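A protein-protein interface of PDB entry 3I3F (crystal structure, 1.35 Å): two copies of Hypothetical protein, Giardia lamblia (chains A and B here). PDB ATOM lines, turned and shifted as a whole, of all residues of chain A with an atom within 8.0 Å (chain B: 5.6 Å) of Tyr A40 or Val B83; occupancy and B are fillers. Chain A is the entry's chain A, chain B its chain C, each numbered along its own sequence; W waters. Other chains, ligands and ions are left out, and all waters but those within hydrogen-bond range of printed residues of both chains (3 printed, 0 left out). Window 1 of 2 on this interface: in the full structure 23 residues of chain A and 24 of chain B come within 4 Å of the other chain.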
ATOM      1  N   PRO A  15      -6.565 -26.495 -18.073  1.00  0.00           N
ATOM      2  CA  PRO A  15      -5.232 -26.064 -18.477  1.00  0.00           C
ATOM      3  C   PRO A  15      -4.562 -25.318 -17.326  1.00  0.00           C
ATOM      4  O   PRO A  15      -5.252 -24.718 -16.499  1.00  0.00           O
ATOM      5  CB  PRO A  15      -5.500 -25.124 -19.655  1.00  0.00           C
ATOM      6  CG  PRO A  15      -6.900 -24.665 -19.476  1.00  0.00           C
ATOM      7  CD  PRO A  15      -7.627 -25.789 -18.814  1.00  0.00           C
ATOM      8  N   THR A  16      -3.238 -25.380 -17.267  1.00  0.00           N
ATOM      9  CA  THR A  16      -2.479 -24.690 -16.234  1.00  0.00           C
ATOM     10  C   THR A  16      -1.551 -23.681 -16.890  1.00  0.00           C
ATOM     11  O   THR A  16      -0.983 -23.950 -17.948  1.00  0.00           O
ATOM     12  CB  THR A  16      -1.662 -25.674 -15.381  1.00  0.00           C
ATOM     13  OG1 THR A  16      -0.804 -26.448 -16.224  1.00  0.00           O
ATOM     14  CG2 THR A  16      -2.585 -26.606 -14.622  1.00  0.00           C
ATOM     15  N   PHE A  17      -1.413 -22.519 -16.262  1.00  0.00           N
ATOM     16  CA  PHE A  17      -0.589 -21.440 -16.792  1.00  0.00           C
ATOM     17  C   PHE A  17       0.598 -21.217 -15.867  1.00  0.00           C
ATOM     18  O   PHE A  17       0.437 -21.106 -14.651  1.00  0.00           O
ATOM     19  CB  PHE A  17      -1.430 -20.176 -16.959  1.00  0.00           C
ATOM     20  CG  PHE A  17      -2.640 -20.386 -17.822  1.00  0.00           C
ATOM     21  CD1 PHE A  17      -2.563 -20.222 -19.200  1.00  0.00           C
ATOM     22  CD2 PHE A  17      -3.845 -20.795 -17.265  1.00  0.00           C
ATOM     23  CE1 PHE A  17      -3.675 -20.440 -20.001  1.00  0.00           C
ATOM     24  CE2 PHE A  17      -4.960 -21.013 -18.059  1.00  0.00           C
ATOM     25  CZ  PHE A  17      -4.874 -20.835 -19.429  1.00  0.00           C
ATOM     26  N   LEU A  18       1.791 -21.187 -16.454  1.00  0.00           N
ATOM     27  CA  LEU A  18       3.040 -21.129 -15.704  1.00  0.00           C
ATOM     28  C   LEU A  18       3.846 -19.905 -16.108  1.00  0.00           C
ATOM     29  O   LEU A  18       3.706 -19.396 -17.224  1.00  0.00           O
ATOM     30  CB  LEU A  18       3.878 -22.384 -15.972  1.00  0.00           C
ATOM     31  CG  LEU A  18       3.472 -23.713 -15.327  1.00  0.00           C
ATOM     32  CD1 LEU A  18       2.057 -24.120 -15.688  1.00  0.00           C
ATOM     33  CD2 LEU A  18       4.451 -24.806 -15.734  1.00  0.00           C
ATOM     34  N   GLY A  30       0.246 -14.866 -21.869  1.00  0.00           N
ATOM     35  CA  GLY A  30       0.533 -16.106 -21.163  1.00  0.00           C
ATOM     36  C   GLY A  30       1.860 -16.635 -21.666  1.00  0.00           C
ATOM     37  O   GLY A  30       2.064 -16.768 -22.873  1.00  0.00           O
ATOM     38  N   GLN A  31       2.777 -16.905 -20.747  1.00  0.00           N
ATOM     39  CA  GLN A  31       4.119 -17.337 -21.116  1.00  0.00           C
ATOM     40  C   GLN A  31       4.133 -18.823 -21.477  1.00  0.00           C
ATOM     41  O   GLN A  31       4.718 -19.225 -22.485  1.00  0.00           O
ATOM     42  CB  GLN A  31       5.080 -17.066 -19.959  1.00  0.00           C
ATOM     43  CG  GLN A  31       6.549 -17.094 -20.333  1.00  0.00           C
ATOM     44  CD  GLN A  31       7.431 -17.190 -19.112  1.00  0.00           C
ATOM     45  OE1 GLN A  31       7.419 -18.203 -18.418  1.00  0.00           O
ATOM     46  NE2 GLN A  31       8.190 -16.131 -18.830  1.00  0.00           N
ATOM     47  N   ILE A  32       3.481 -19.623 -20.635  1.00  0.00           N
ATOM     48  CA  ILE A  32       3.471 -21.075 -20.751  1.00  0.00           C
ATOM     49  C   ILE A  32       2.082 -21.581 -20.380  1.00  0.00           C
ATOM     50  O   ILE A  32       1.522 -21.151 -19.373  1.00  0.00           O
ATOM     51  CB  ILE A  32       4.474 -21.732 -19.769  1.00  0.00           C
ATOM     52  CG1 ILE A  32       5.870 -21.117 -19.896  1.00  0.00           C
ATOM     53  CG2 ILE A  32       4.533 -23.242 -19.989  1.00  0.00           C
ATOM     54  CD1 ILE A  32       6.846 -21.625 -18.859  1.00  0.00           C
ATOM     55  N   ALA A  33       1.530 -22.484 -21.186  1.00  0.00           N
ATOM     56  CA  ALA A  33       0.298 -23.185 -20.833  1.00  0.00           C
ATOM     57  C   ALA A  33       0.510 -24.685 -21.002  1.00  0.00           C
ATOM     58  O   ALA A  33       1.122 -25.119 -21.977  1.00  0.00           O
ATOM     59  CB  ALA A  33      -0.853 -22.712 -21.691  1.00  0.00           C
ATOM     60  N   VAL A  34       0.016 -25.468 -20.045  1.00  0.00           N
ATOM     61  CA  VAL A  34       0.094 -26.924 -20.114  1.00  0.00           C
ATOM     62  C   VAL A  34      -1.314 -27.511 -20.088  1.00  0.00           C
ATOM     63  O   VAL A  34      -2.132 -27.139 -19.248  1.00  0.00           O
ATOM     64  CB  VAL A  34       0.911 -27.510 -18.944  1.00  0.00           C
ATOM     65  CG1 VAL A  34       0.969 -29.032 -19.038  1.00  0.00           C
ATOM     66  CG2 VAL A  34       2.314 -26.917 -18.920  1.00  0.00           C
ATOM     67  N   VAL A  35      -1.588 -28.421 -21.019  1.00  0.00           N
ATOM     68  CA  VAL A  35      -2.889 -29.083 -21.109  1.00  0.00           C
ATOM     69  C   VAL A  35      -2.717 -30.493 -21.676  1.00  0.00           C
ATOM     70  O   VAL A  35      -2.163 -30.667 -22.760  1.00  0.00           O
ATOM     71  CB  VAL A  35      -3.880 -28.275 -21.991  1.00  0.00           C
ATOM     72  CG1 VAL A  35      -3.279 -27.977 -23.360  1.00  0.00           C
ATOM     73  CG2 VAL A  35      -5.208 -29.010 -22.129  1.00  0.00           C
ATOM     74  N   ASN A  36      -3.175 -31.492 -20.923  1.00  0.00           N
ATOM     75  CA  ASN A  36      -3.170 -32.889 -21.372  1.00  0.00           C
ATOM     76  C   ASN A  36      -1.809 -33.366 -21.896  1.00  0.00           C
ATOM     77  O   ASN A  36      -1.728 -33.991 -22.952  1.00  0.00           O
ATOM     78  CB  ASN A  36      -4.245 -33.102 -22.448  1.00  0.00           C
ATOM     79  CG  ASN A  36      -5.618 -32.623 -22.012  1.00  0.00           C
ATOM     80  OD1 ASN A  36      -5.960 -32.668 -20.830  1.00  0.00           O
ATOM     81  ND2 ASN A  36      -6.414 -32.161 -22.970  1.00  0.00           N
ATOM     82  N   GLY A  37      -0.747 -33.058 -21.158  1.00  0.00           N
ATOM     83  CA  GLY A  37       0.600 -33.489 -21.533  1.00  0.00           C
ATOM     84  C   GLY A  37       1.234 -32.726 -22.687  1.00  0.00           C
ATOM     85  O   GLY A  37       2.257 -33.154 -23.222  1.00  0.00           O
ATOM     86  N   MET A  38       0.636 -31.597 -23.070  1.00  0.00           N
ATOM     87  CA  MET A  38       1.175 -30.742 -24.124  1.00  0.00           C
ATOM     88  C   MET A  38       1.468 -29.356 -23.564  1.00  0.00           C
ATOM     89  O   MET A  38       0.723 -28.849 -22.722  1.00  0.00           O
ATOM     90  CB  MET A  38       0.188 -30.630 -25.286  1.00  0.00           C
ATOM     91  CG  MET A  38      -0.123 -31.952 -25.981  1.00  0.00           C
ATOM     92  SD  MET A  38       1.305 -32.711 -26.784  1.00  0.00           S
ATOM     93  CE  MET A  38       1.659 -31.517 -28.068  1.00  0.00           C
ATOM     94  N   VAL A  39       2.555 -28.754 -24.040  1.00  0.00           N
ATOM     95  CA  VAL A  39       2.968 -27.423 -23.614  1.00  0.00           C
ATOM     96  C   VAL A  39       2.832 -26.446 -24.778  1.00  0.00           C
ATOM     97  O   VAL A  39       3.251 -26.746 -25.898  1.00  0.00           O
ATOM     98  CB  VAL A  39       4.430 -27.421 -23.128  1.00  0.00           C
ATOM     99  CG1 VAL A  39       4.805 -26.056 -22.552  1.00  0.00           C
ATOM    100  CG2 VAL A  39       4.654 -28.521 -22.096  1.00  0.00           C
ATOM    101  N   TYR A  40       2.225 -25.293 -24.502  1.00  0.00           N
ATOM    102  CA  TYR A  40       2.103 -24.196 -25.460  1.00  0.00           C
ATOM    103  C   TYR A  40       2.838 -22.993 -24.888  1.00  0.00           C
ATOM    104  O   TYR A  40       2.816 -22.775 -23.679  1.00  0.00           O
ATOM    105  CB  TYR A  40       0.632 -23.828 -25.673  1.00  0.00           C
ATOM    106  CG  TYR A  40      -0.177 -24.902 -26.360  1.00  0.00           C
ATOM    107  CD1 TYR A  40      -0.509 -24.794 -27.705  1.00  0.00           C
ATOM    108  CD2 TYR A  40      -0.607 -26.029 -25.665  1.00  0.00           C
ATOM    109  CE1 TYR A  40      -1.248 -25.778 -28.344  1.00  0.00           C
ATOM    110  CE2 TYR A  40      -1.345 -27.024 -26.297  1.00  0.00           C
ATOM    111  CZ  TYR A  40      -1.663 -26.888 -27.637  1.00  0.00           C
ATOM    112  OH  TYR A  40      -2.395 -27.860 -28.279  1.00  0.00           O
ATOM    113  N   LEU A  41       3.487 -22.214 -25.749  1.00  0.00           N
ATOM    114  CA  LEU A  41       4.164 -20.993 -25.312  1.00  0.00           C
ATOM    115  C   LEU A  41       3.561 -19.754 -25.959  1.00  0.00           C
ATOM    116  O   LEU A  41       3.153 -19.780 -27.122  1.00  0.00           O
ATOM    117  CB  LEU A  41       5.654 -21.035 -25.653  1.00  0.00           C
ATOM    118  CG  LEU A  41       6.500 -22.186 -25.109  1.00  0.00           C
ATOM    119  CD1 LEU A  41       7.959 -21.952 -25.464  1.00  0.00           C
ATOM    120  CD2 LEU A  41       6.347 -22.337 -23.606  1.00  0.00           C
ATOM    121  N   GLY A  42       3.529 -18.660 -25.203  1.00  0.00           N
ATOM    122  CA  GLY A  42       3.258 -17.350 -25.777  1.00  0.00           C
ATOM    123  C   GLY A  42       4.435 -16.919 -26.632  1.00  0.00           C
ATOM    124  O   GLY A  42       5.494 -17.559 -26.616  1.00  0.00           O
ATOM    125  N   GLY A  43       4.259 -15.838 -27.380  1.00  0.00           N
ATOM    126  CA  GLY A  43       5.310 -15.341 -28.264  1.00  0.00           C
ATOM    127  C   GLY A  43       6.616 -15.127 -27.524  1.00  0.00           C
ATOM    128  O   GLY A  43       6.623 -14.595 -26.410  1.00  0.00           O
ATOM    129  N   CYS A  71      11.662 -21.974 -20.719  1.00  0.00           N
ATOM    130  CA  CYS A  71      10.224 -22.150 -20.507  1.00  0.00           C
ATOM    131  C   CYS A  71       9.815 -23.615 -20.627  1.00  0.00           C
ATOM    132  O   CYS A  71       9.092 -24.132 -19.774  1.00  0.00           O
ATOM    133  CB  CYS A  71       9.415 -21.310 -21.496  1.00  0.00           C
ATOM    134  SG  CYS A  71       9.411 -19.547 -21.140  1.00  0.00           S
ATOM    135  N   LEU A  72      10.278 -24.284 -21.681  1.00  0.00           N
ATOM    136  CA  LEU A  72       9.919 -25.681 -21.910  1.00  0.00           C
ATOM    137  C   LEU A  72      10.446 -26.599 -20.807  1.00  0.00           C
ATOM    138  O   LEU A  72       9.725 -27.475 -20.338  1.00  0.00           O
ATOM    139  CB  LEU A  72      10.405 -26.158 -23.284  1.00  0.00           C
ATOM    140  CG  LEU A  72       9.671 -25.539 -24.477  1.00  0.00           C
ATOM    141  CD1 LEU A  72      10.293 -25.986 -25.789  1.00  0.00           C
ATOM    142  CD2 LEU A  72       8.192 -25.896 -24.444  1.00  0.00           C
ATOM    143  N   ALA A  75       8.460 -26.323 -17.757  1.00  0.00           N
ATOM    144  CA  ALA A  75       7.166 -26.991 -17.937  1.00  0.00           C
ATOM    145  C   ALA A  75       7.283 -28.507 -18.169  1.00  0.00           C
ATOM    146  O   ALA A  75       6.361 -29.119 -18.708  1.00  0.00           O
ATOM    147  CB  ALA A  75       6.415 -26.342 -19.100  1.00  0.00           C
ATOM    148  N   SER A  77       9.306 -30.174 -20.201  1.00  0.00           N
ATOM    149  CA  SER A  77       9.477 -30.445 -21.623  1.00  0.00           C
ATOM    150  C   SER A  77      10.915 -30.090 -22.007  1.00  0.00           C
ATOM    151  O   SER A  77      11.810 -30.106 -21.162  1.00  0.00           O
ATOM    152  CB  SER A  77       8.459 -29.630 -22.433  1.00  0.00           C
ATOM    153  OG  SER A  77       8.463 -29.990 -23.805  1.00  0.00           O
ATOM    154  N   ASN A 135       3.593 -19.837 -31.471  1.00  0.00           N
ATOM    155  CA  ASN A 135       2.924 -21.129 -31.627  1.00  0.00           C
ATOM    156  C   ASN A 135       3.848 -22.326 -31.395  1.00  0.00           C
ATOM    157  O   ASN A 135       3.745 -23.344 -32.082  1.00  0.00           O
ATOM    158  CB  ASN A 135       2.246 -21.219 -33.001  1.00  0.00           C
ATOM    159  CG  ASN A 135       1.114 -20.227 -33.153  1.00  0.00           C
ATOM    160  OD1 ASN A 135       0.362 -19.985 -32.210  1.00  0.00           O
ATOM    161  ND2 ASN A 135       0.986 -19.644 -34.337  1.00  0.00           N
ATOM    162  N   VAL A 136       4.745 -22.204 -30.419  1.00  0.00           N
ATOM    163  CA  VAL A 136       5.562 -23.337 -30.008  1.00  0.00           C
ATOM    164  C   VAL A 136       4.650 -24.328 -29.302  1.00  0.00           C
ATOM    165  O   VAL A 136       3.988 -23.978 -28.323  1.00  0.00           O
ATOM    166  CB  VAL A 136       6.706 -22.926 -29.064  1.00  0.00           C
ATOM    167  CG1 VAL A 136       7.409 -24.160 -28.502  1.00  0.00           C
ATOM    168  CG2 VAL A 136       7.695 -22.035 -29.795  1.00  0.00           C
ATOM    169  N   VAL A 137       4.601 -25.546 -29.832  1.00  0.00           N
ATOM    170  CA  VAL A 137       3.826 -26.639 -29.259  1.00  0.00           C
ATOM    171  C   VAL A 137       4.790 -27.791 -29.002  1.00  0.00           C
ATOM    172  O   VAL A 137       5.536 -28.194 -29.899  1.00  0.00           O
ATOM    173  CB  VAL A 137       2.709 -27.096 -30.221  1.00  0.00           C
ATOM    174  CG1 VAL A 137       1.876 -28.214 -29.596  1.00  0.00           C
ATOM    175  CG2 VAL A 137       1.823 -25.913 -30.603  1.00  0.00           C
ATOM    176  N   ALA A 138       4.784 -28.308 -27.777  1.00  0.00           N
ATOM    177  CA  ALA A 138       5.719 -29.355 -27.370  1.00  0.00           C
ATOM    178  C   ALA A 138       5.033 -30.391 -26.492  1.00  0.00           C
ATOM    179  O   ALA A 138       4.053 -30.092 -25.814  1.00  0.00           O
ATOM    180  CB  ALA A 138       6.894 -28.741 -26.627  1.00  0.00           C
ATOM    181  N   ALA A 139       5.556 -31.613 -26.518  1.00  0.00           N
ATOM    182  CA  ALA A 139       5.093 -32.678 -25.634  1.00  0.00           C
ATOM    183  C   ALA A 139       5.831 -32.598 -24.303  1.00  0.00           C
ATOM    184  O   ALA A 139       6.988 -32.184 -24.251  1.00  0.00           O
ATOM    185  CB  ALA A 139       5.324 -34.036 -26.281  1.00  0.00           C
ATOM    186  N   GLN A 140       5.158 -32.989 -23.226  1.00  0.00           N
ATOM    187  CA  GLN A 140       5.817 -33.131 -21.929  1.00  0.00           C
ATOM    188  C   GLN A 140       6.578 -34.454 -21.870  1.00  0.00           C
ATOM    189  O   GLN A 140       6.285 -35.387 -22.622  1.00  0.00           O
ATOM    190  CB  GLN A 140       4.806 -33.061 -20.784  1.00  0.00           C
ATOM    191  CG  GLN A 140       4.373 -31.652 -20.428  1.00  0.00           C
ATOM    192  CD  GLN A 140       3.590 -31.596 -19.130  1.00  0.00           C
ATOM    193  OE1 GLN A 140       2.640 -32.353 -18.933  1.00  0.00           O
ATOM    194  NE2 GLN A 140       3.982 -30.695 -18.239  1.00  0.00           N
ATOM    195  N   MET B  38     -10.425 -31.198 -26.885  1.00  0.00           N
ATOM    196  CA  MET B  38      -9.897 -29.880 -27.237  1.00  0.00           C
ATOM    197  C   MET B  38     -10.802 -29.237 -28.278  1.00  0.00           C
ATOM    198  O   MET B  38     -11.403 -29.930 -29.101  1.00  0.00           O
ATOM    199  CB  MET B  38      -8.475 -29.992 -27.792  1.00  0.00           C
ATOM    200  CG  MET B  38      -7.456 -30.571 -26.812  1.00  0.00           C
ATOM    201  SD  MET B  38      -7.163 -29.540 -25.358  1.00  0.00           S
ATOM    202  CE  MET B  38      -6.367 -28.111 -26.089  1.00  0.00           C
ATOM    203  N   TYR B  40     -10.929 -26.270 -31.299  1.00  0.00           N
ATOM    204  CA  TYR B  40     -10.219 -25.379 -32.211  1.00  0.00           C
ATOM    205  C   TYR B  40     -11.241 -24.483 -32.899  1.00  0.00           C
ATOM    206  O   TYR B  40     -12.345 -24.928 -33.203  1.00  0.00           O
ATOM    207  CB  TYR B  40      -9.467 -26.184 -33.272  1.00  0.00           C
ATOM    208  CG  TYR B  40      -8.292 -26.986 -32.749  1.00  0.00           C
ATOM    209  CD1 TYR B  40      -6.984 -26.571 -32.984  1.00  0.00           C
ATOM    210  CD2 TYR B  40      -8.486 -28.166 -32.033  1.00  0.00           C
ATOM    211  CE1 TYR B  40      -5.899 -27.303 -32.515  1.00  0.00           C
ATOM    212  CE2 TYR B  40      -7.404 -28.905 -31.554  1.00  0.00           C
ATOM    213  CZ  TYR B  40      -6.114 -28.466 -31.801  1.00  0.00           C
ATOM    214  OH  TYR B  40      -5.036 -29.188 -31.338  1.00  0.00           O
ATOM    215  N   TYR B  81     -10.780 -21.241 -20.567  1.00  0.00           N
ATOM    216  CA  TYR B  81     -10.100 -22.493 -20.926  1.00  0.00           C
ATOM    217  C   TYR B  81      -9.305 -22.408 -22.238  1.00  0.00           C
ATOM    218  O   TYR B  81      -8.799 -23.420 -22.727  1.00  0.00           O
ATOM    219  CB  TYR B  81     -11.104 -23.655 -20.961  1.00  0.00           C
ATOM    220  CG  TYR B  81     -11.198 -24.385 -19.639  1.00  0.00           C
ATOM    221  CD1 TYR B  81     -11.294 -23.685 -18.442  1.00  0.00           C
ATOM    222  CD2 TYR B  81     -11.188 -25.773 -19.581  1.00  0.00           C
ATOM    223  CE1 TYR B  81     -11.375 -24.344 -17.229  1.00  0.00           C
ATOM    224  CE2 TYR B  81     -11.270 -26.441 -18.369  1.00  0.00           C
ATOM    225  CZ  TYR B  81     -11.362 -25.720 -17.198  1.00  0.00           C
ATOM    226  OH  TYR B  81     -11.446 -26.374 -15.990  1.00  0.00           O
ATOM    227  N   ILE B  82      -9.172 -21.202 -22.788  1.00  0.00           N
ATOM    228  CA  ILE B  82      -8.293 -20.988 -23.937  1.00  0.00           C
ATOM    229  C   ILE B  82      -6.839 -21.158 -23.501  1.00  0.00           C
ATOM    230  O   ILE B  82      -6.422 -20.581 -22.493  1.00  0.00           O
ATOM    231  CB  ILE B  82      -8.466 -19.582 -24.545  1.00  0.00           C
ATOM    232  CG1 ILE B  82      -9.874 -19.414 -25.129  1.00  0.00           C
ATOM    233  CG2 ILE B  82      -7.414 -19.338 -25.623  1.00  0.00           C
ATOM    234  CD1 ILE B  82     -10.148 -18.017 -25.663  1.00  0.00           C
ATOM    235  N   VAL B  83      -6.085 -21.962 -24.250  1.00  0.00           N
ATOM    236  CA  VAL B  83      -4.663 -22.187 -23.977  1.00  0.00           C
ATOM    237  C   VAL B  83      -3.791 -21.248 -24.810  1.00  0.00           C
ATOM    238  O   VAL B  83      -2.759 -20.759 -24.339  1.00  0.00           O
ATOM    239  CB  VAL B  83      -4.253 -23.662 -24.244  1.00  0.00           C
ATOM    240  CG1 VAL B  83      -4.582 -24.079 -25.665  1.00  0.00           C
ATOM    241  CG2 VAL B  83      -2.773 -23.871 -23.969  1.00  0.00           C
ATOM    242  N   SER B  84      -4.205 -20.999 -26.050  1.00  0.00           N
ATOM    243  CA  SER B  84      -3.417 -20.186 -26.971  1.00  0.00           C
ATOM    244  C   SER B  84      -4.297 -19.519 -28.023  1.00  0.00           C
ATOM    245  O   SER B  84      -5.327 -20.066 -28.412  1.00  0.00           O
ATOM    246  CB  SER B  84      -2.366 -21.068 -27.652  1.00  0.00           C
ATOM    247  OG  SER B  84      -1.509 -20.318 -28.494  1.00  0.00           O
ATOM    248  N   LEU B  85      -3.885 -18.333 -28.463  1.00  0.00           N
ATOM    249  CA  LEU B  85      -4.508 -17.650 -29.595  1.00  0.00           C
ATOM    250  C   LEU B  85      -3.483 -16.738 -30.271  1.00  0.00           C
ATOM    251  O   LEU B  85      -2.436 -16.438 -29.692  1.00  0.00           O
ATOM    252  CB  LEU B  85      -5.748 -16.863 -29.148  1.00  0.00           C
ATOM    253  CG  LEU B  85      -5.583 -15.772 -28.084  1.00  0.00           C
ATOM    254  CD1 LEU B  85      -4.992 -14.499 -28.672  1.00  0.00           C
ATOM    255  CD2 LEU B  85      -6.922 -15.456 -27.426  1.00  0.00           C
ATOM    256  N   PRO B 116      -4.194 -16.391 -21.745  1.00  0.00           N
ATOM    257  CA  PRO B 116      -3.692 -17.442 -22.623  1.00  0.00           C
ATOM    258  C   PRO B 116      -2.381 -17.074 -23.306  1.00  0.00           C
ATOM    259  O   PRO B 116      -2.008 -15.902 -23.368  1.00  0.00           O
ATOM    260  CB  PRO B 116      -4.810 -17.594 -23.662  1.00  0.00           C
ATOM    261  CG  PRO B 116      -5.498 -16.286 -23.678  1.00  0.00           C
ATOM    262  CD  PRO B 116      -5.419 -15.764 -22.276  1.00  0.00           C
ATOM    263  N   CYS B 117      -1.681 -18.082 -23.807  1.00  0.00           N
ATOM    264  CA  CYS B 117      -0.549 -17.841 -24.681  1.00  0.00           C
ATOM    265  C   CYS B 117      -1.042 -17.000 -25.840  1.00  0.00           C
ATOM    266  O   CYS B 117      -2.128 -17.246 -26.373  1.00  0.00           O
ATOM    267  CB  CYS B 117       0.030 -19.148 -25.207  1.00  0.00           C
ATOM    268  SG  CYS B 117       0.706 -20.198 -23.927  1.00  0.00           S
ATOM    269  N   VAL B 137      -7.069 -22.187 -29.499  1.00  0.00           N
ATOM    270  CA  VAL B 137      -7.077 -23.566 -29.033  1.00  0.00           C
ATOM    271  C   VAL B 137      -7.508 -23.539 -27.574  1.00  0.00           C
ATOM    272  O   VAL B 137      -6.952 -22.783 -26.777  1.00  0.00           O
ATOM    273  CB  VAL B 137      -5.680 -24.214 -29.146  1.00  0.00           C
ATOM    274  CG1 VAL B 137      -5.714 -25.650 -28.633  1.00  0.00           C
ATOM    275  CG2 VAL B 137      -5.176 -24.168 -30.586  1.00  0.00           C
ATOM    276  N   ALA B 138      -8.507 -24.348 -27.230  1.00  0.00           N
ATOM    277  CA  ALA B 138      -9.075 -24.346 -25.885  1.00  0.00           C
ATOM    278  C   ALA B 138      -9.392 -25.764 -25.425  1.00  0.00           C
ATOM    279  O   ALA B 138      -9.595 -26.659 -26.242  1.00  0.00           O
ATOM    280  CB  ALA B 138     -10.331 -23.487 -25.849  1.00  0.00           C
ATOM    281  N   ALA B 139      -9.429 -25.959 -24.112  1.00  0.00           N
ATOM    282  CA  ALA B 139      -9.820 -27.240 -23.532  1.00  0.00           C
ATOM    283  C   ALA B 139     -11.318 -27.242 -23.253  1.00  0.00           C
ATOM    284  O   ALA B 139     -11.897 -26.202 -22.949  1.00  0.00           O
ATOM    285  CB  ALA B 139      -9.045 -27.494 -22.250  1.00  0.00           C
HETATM  286  O   HOH W   1       1.610 -21.828 -28.510  1.00  0.00           O
HETATM  287  O   HOH W   2      -2.554 -28.102 -31.000  1.00  0.00           O
HETATM  288  O   HOH W   3      -2.462 -20.741 -31.016  1.00  0.00           O
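Hydrophobic or aromatic side chains of chain B that line the printed part of chain A: Met B38, Tyr B81 and Val B83.
Along chain B the printed residues that touch a printed residue of chain A span positions 38 to 117.
Of the 28 printed residues of chain A, 9 touch a printed residue of chain B.
Printed residues of chain A that touch a printed residue of chain B: Pro A15, Phe A17, Gly A30, Ala A33, Val A35, Asn A36, Tyr A40, Leu A41 and Gly A42.
Among the printed residues, 13 pairs touch across the chains.
Water W3 lies within hydrogen-bond range of the side-chain hydroxyl of Ser B84 (2.7 Å) and the side-chain amide oxygen of Asn A135 (3.2 Å).
Water W2 bridges OH of Tyr B40 and OH of Tyr A40.
Water W1 lies within hydrogen-bond range of O of Leu A41 (2.9 Å), O of Val A136 (3.2 Å) and OG of Ser B84 (3.5 Å).
O of Pro B116 sits at hydrogen-bond distance from N of Gly A30, 2.9 Å away.
The side-chain sulfur of Cys B117 sits at hydrogen-bond distance from the backbone NH of Ala A33.
The side-chain amide nitrogen (ND2) of Asn A36 is in hydrogen-bond range of the side-chain sulfur (SD) of Met B38 (3.6 Å).
O of Tyr A40 is in hydrogen-bond range of SG of Cys B117, 3.3 Å away.
The backbone NH of Gly A42 lies within hydrogen-bond range of the side-chain sulfur of Cys B117, at 3.5 Å.
Printed residues of chain B within 4 Å of Tyr A40: Val B83 (3.5 Å) and Cys B117 (3.3 Å).
Of the printed residues of chain A, Val B83 touches Ala A33 and Tyr A40.
Of the printed residues of chain B, Asn A36 touches Met B38.
Of the printed residues of chain B, Leu A41 touches Cys B117 (3.5 Å).
Of the printed residues of chain B, Gly A42 touches Cys B117 (3.5 Å).
Printed residues of chain A within 4 Å of Met B38: Val A35 and Asn A36.
Of the printed residues of chain A, Ile B82 touches Phe A17.
Ala B139 touches none of the printed residues of chain A.
Ala A75 touches none of the printed residues of chain B.
Among the printed residues, pairs that only touch across the chains: Pro A15 with Tyr B81 (3.6 Å), Phe A17 with Ile B82 (3.4 Å), Phe A17 with Pro B116 (3.98 Å), Gly A30 with Cys B117 (3.4 Å), Ala A33 with Val B83 (3.2 Å), Val A35 with Met B38 (3.8 Å), Tyr A40 with Val B83 (3.5 Å) and Leu A41 with Cys B117 (3.5 Å).
N of Gly A42 lies within hydrogen-bond range of O of Gln A31 (3.0 Å).
The backbone NH (N) of Leu A41 sits at hydrogen-bond distance from the backbone carbonyl oxygen (O) of Val A136 (3.2 Å).
The backbone carbonyl oxygen (O) of Tyr B81 sits at hydrogen-bond distance from the backbone NH (N) of Ala B139 (3.0 Å).
The backbone NH (N) of Cys B117 is in hydrogen-bond range of the backbone carbonyl oxygen (O) of Val B83.
The backbone NH (N) of Val B83 sits at hydrogen-bond distance from the backbone carbonyl oxygen (O) of Val B137 (2.8 Å).
N of Leu B85 lies within hydrogen-bond range of O of Cys B117 (2.9 Å).
5 positions are printed for both chains.
Of the 13 pairs that touch across the chains among the printed residues, none has its exchanged pair printed and touching as well.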
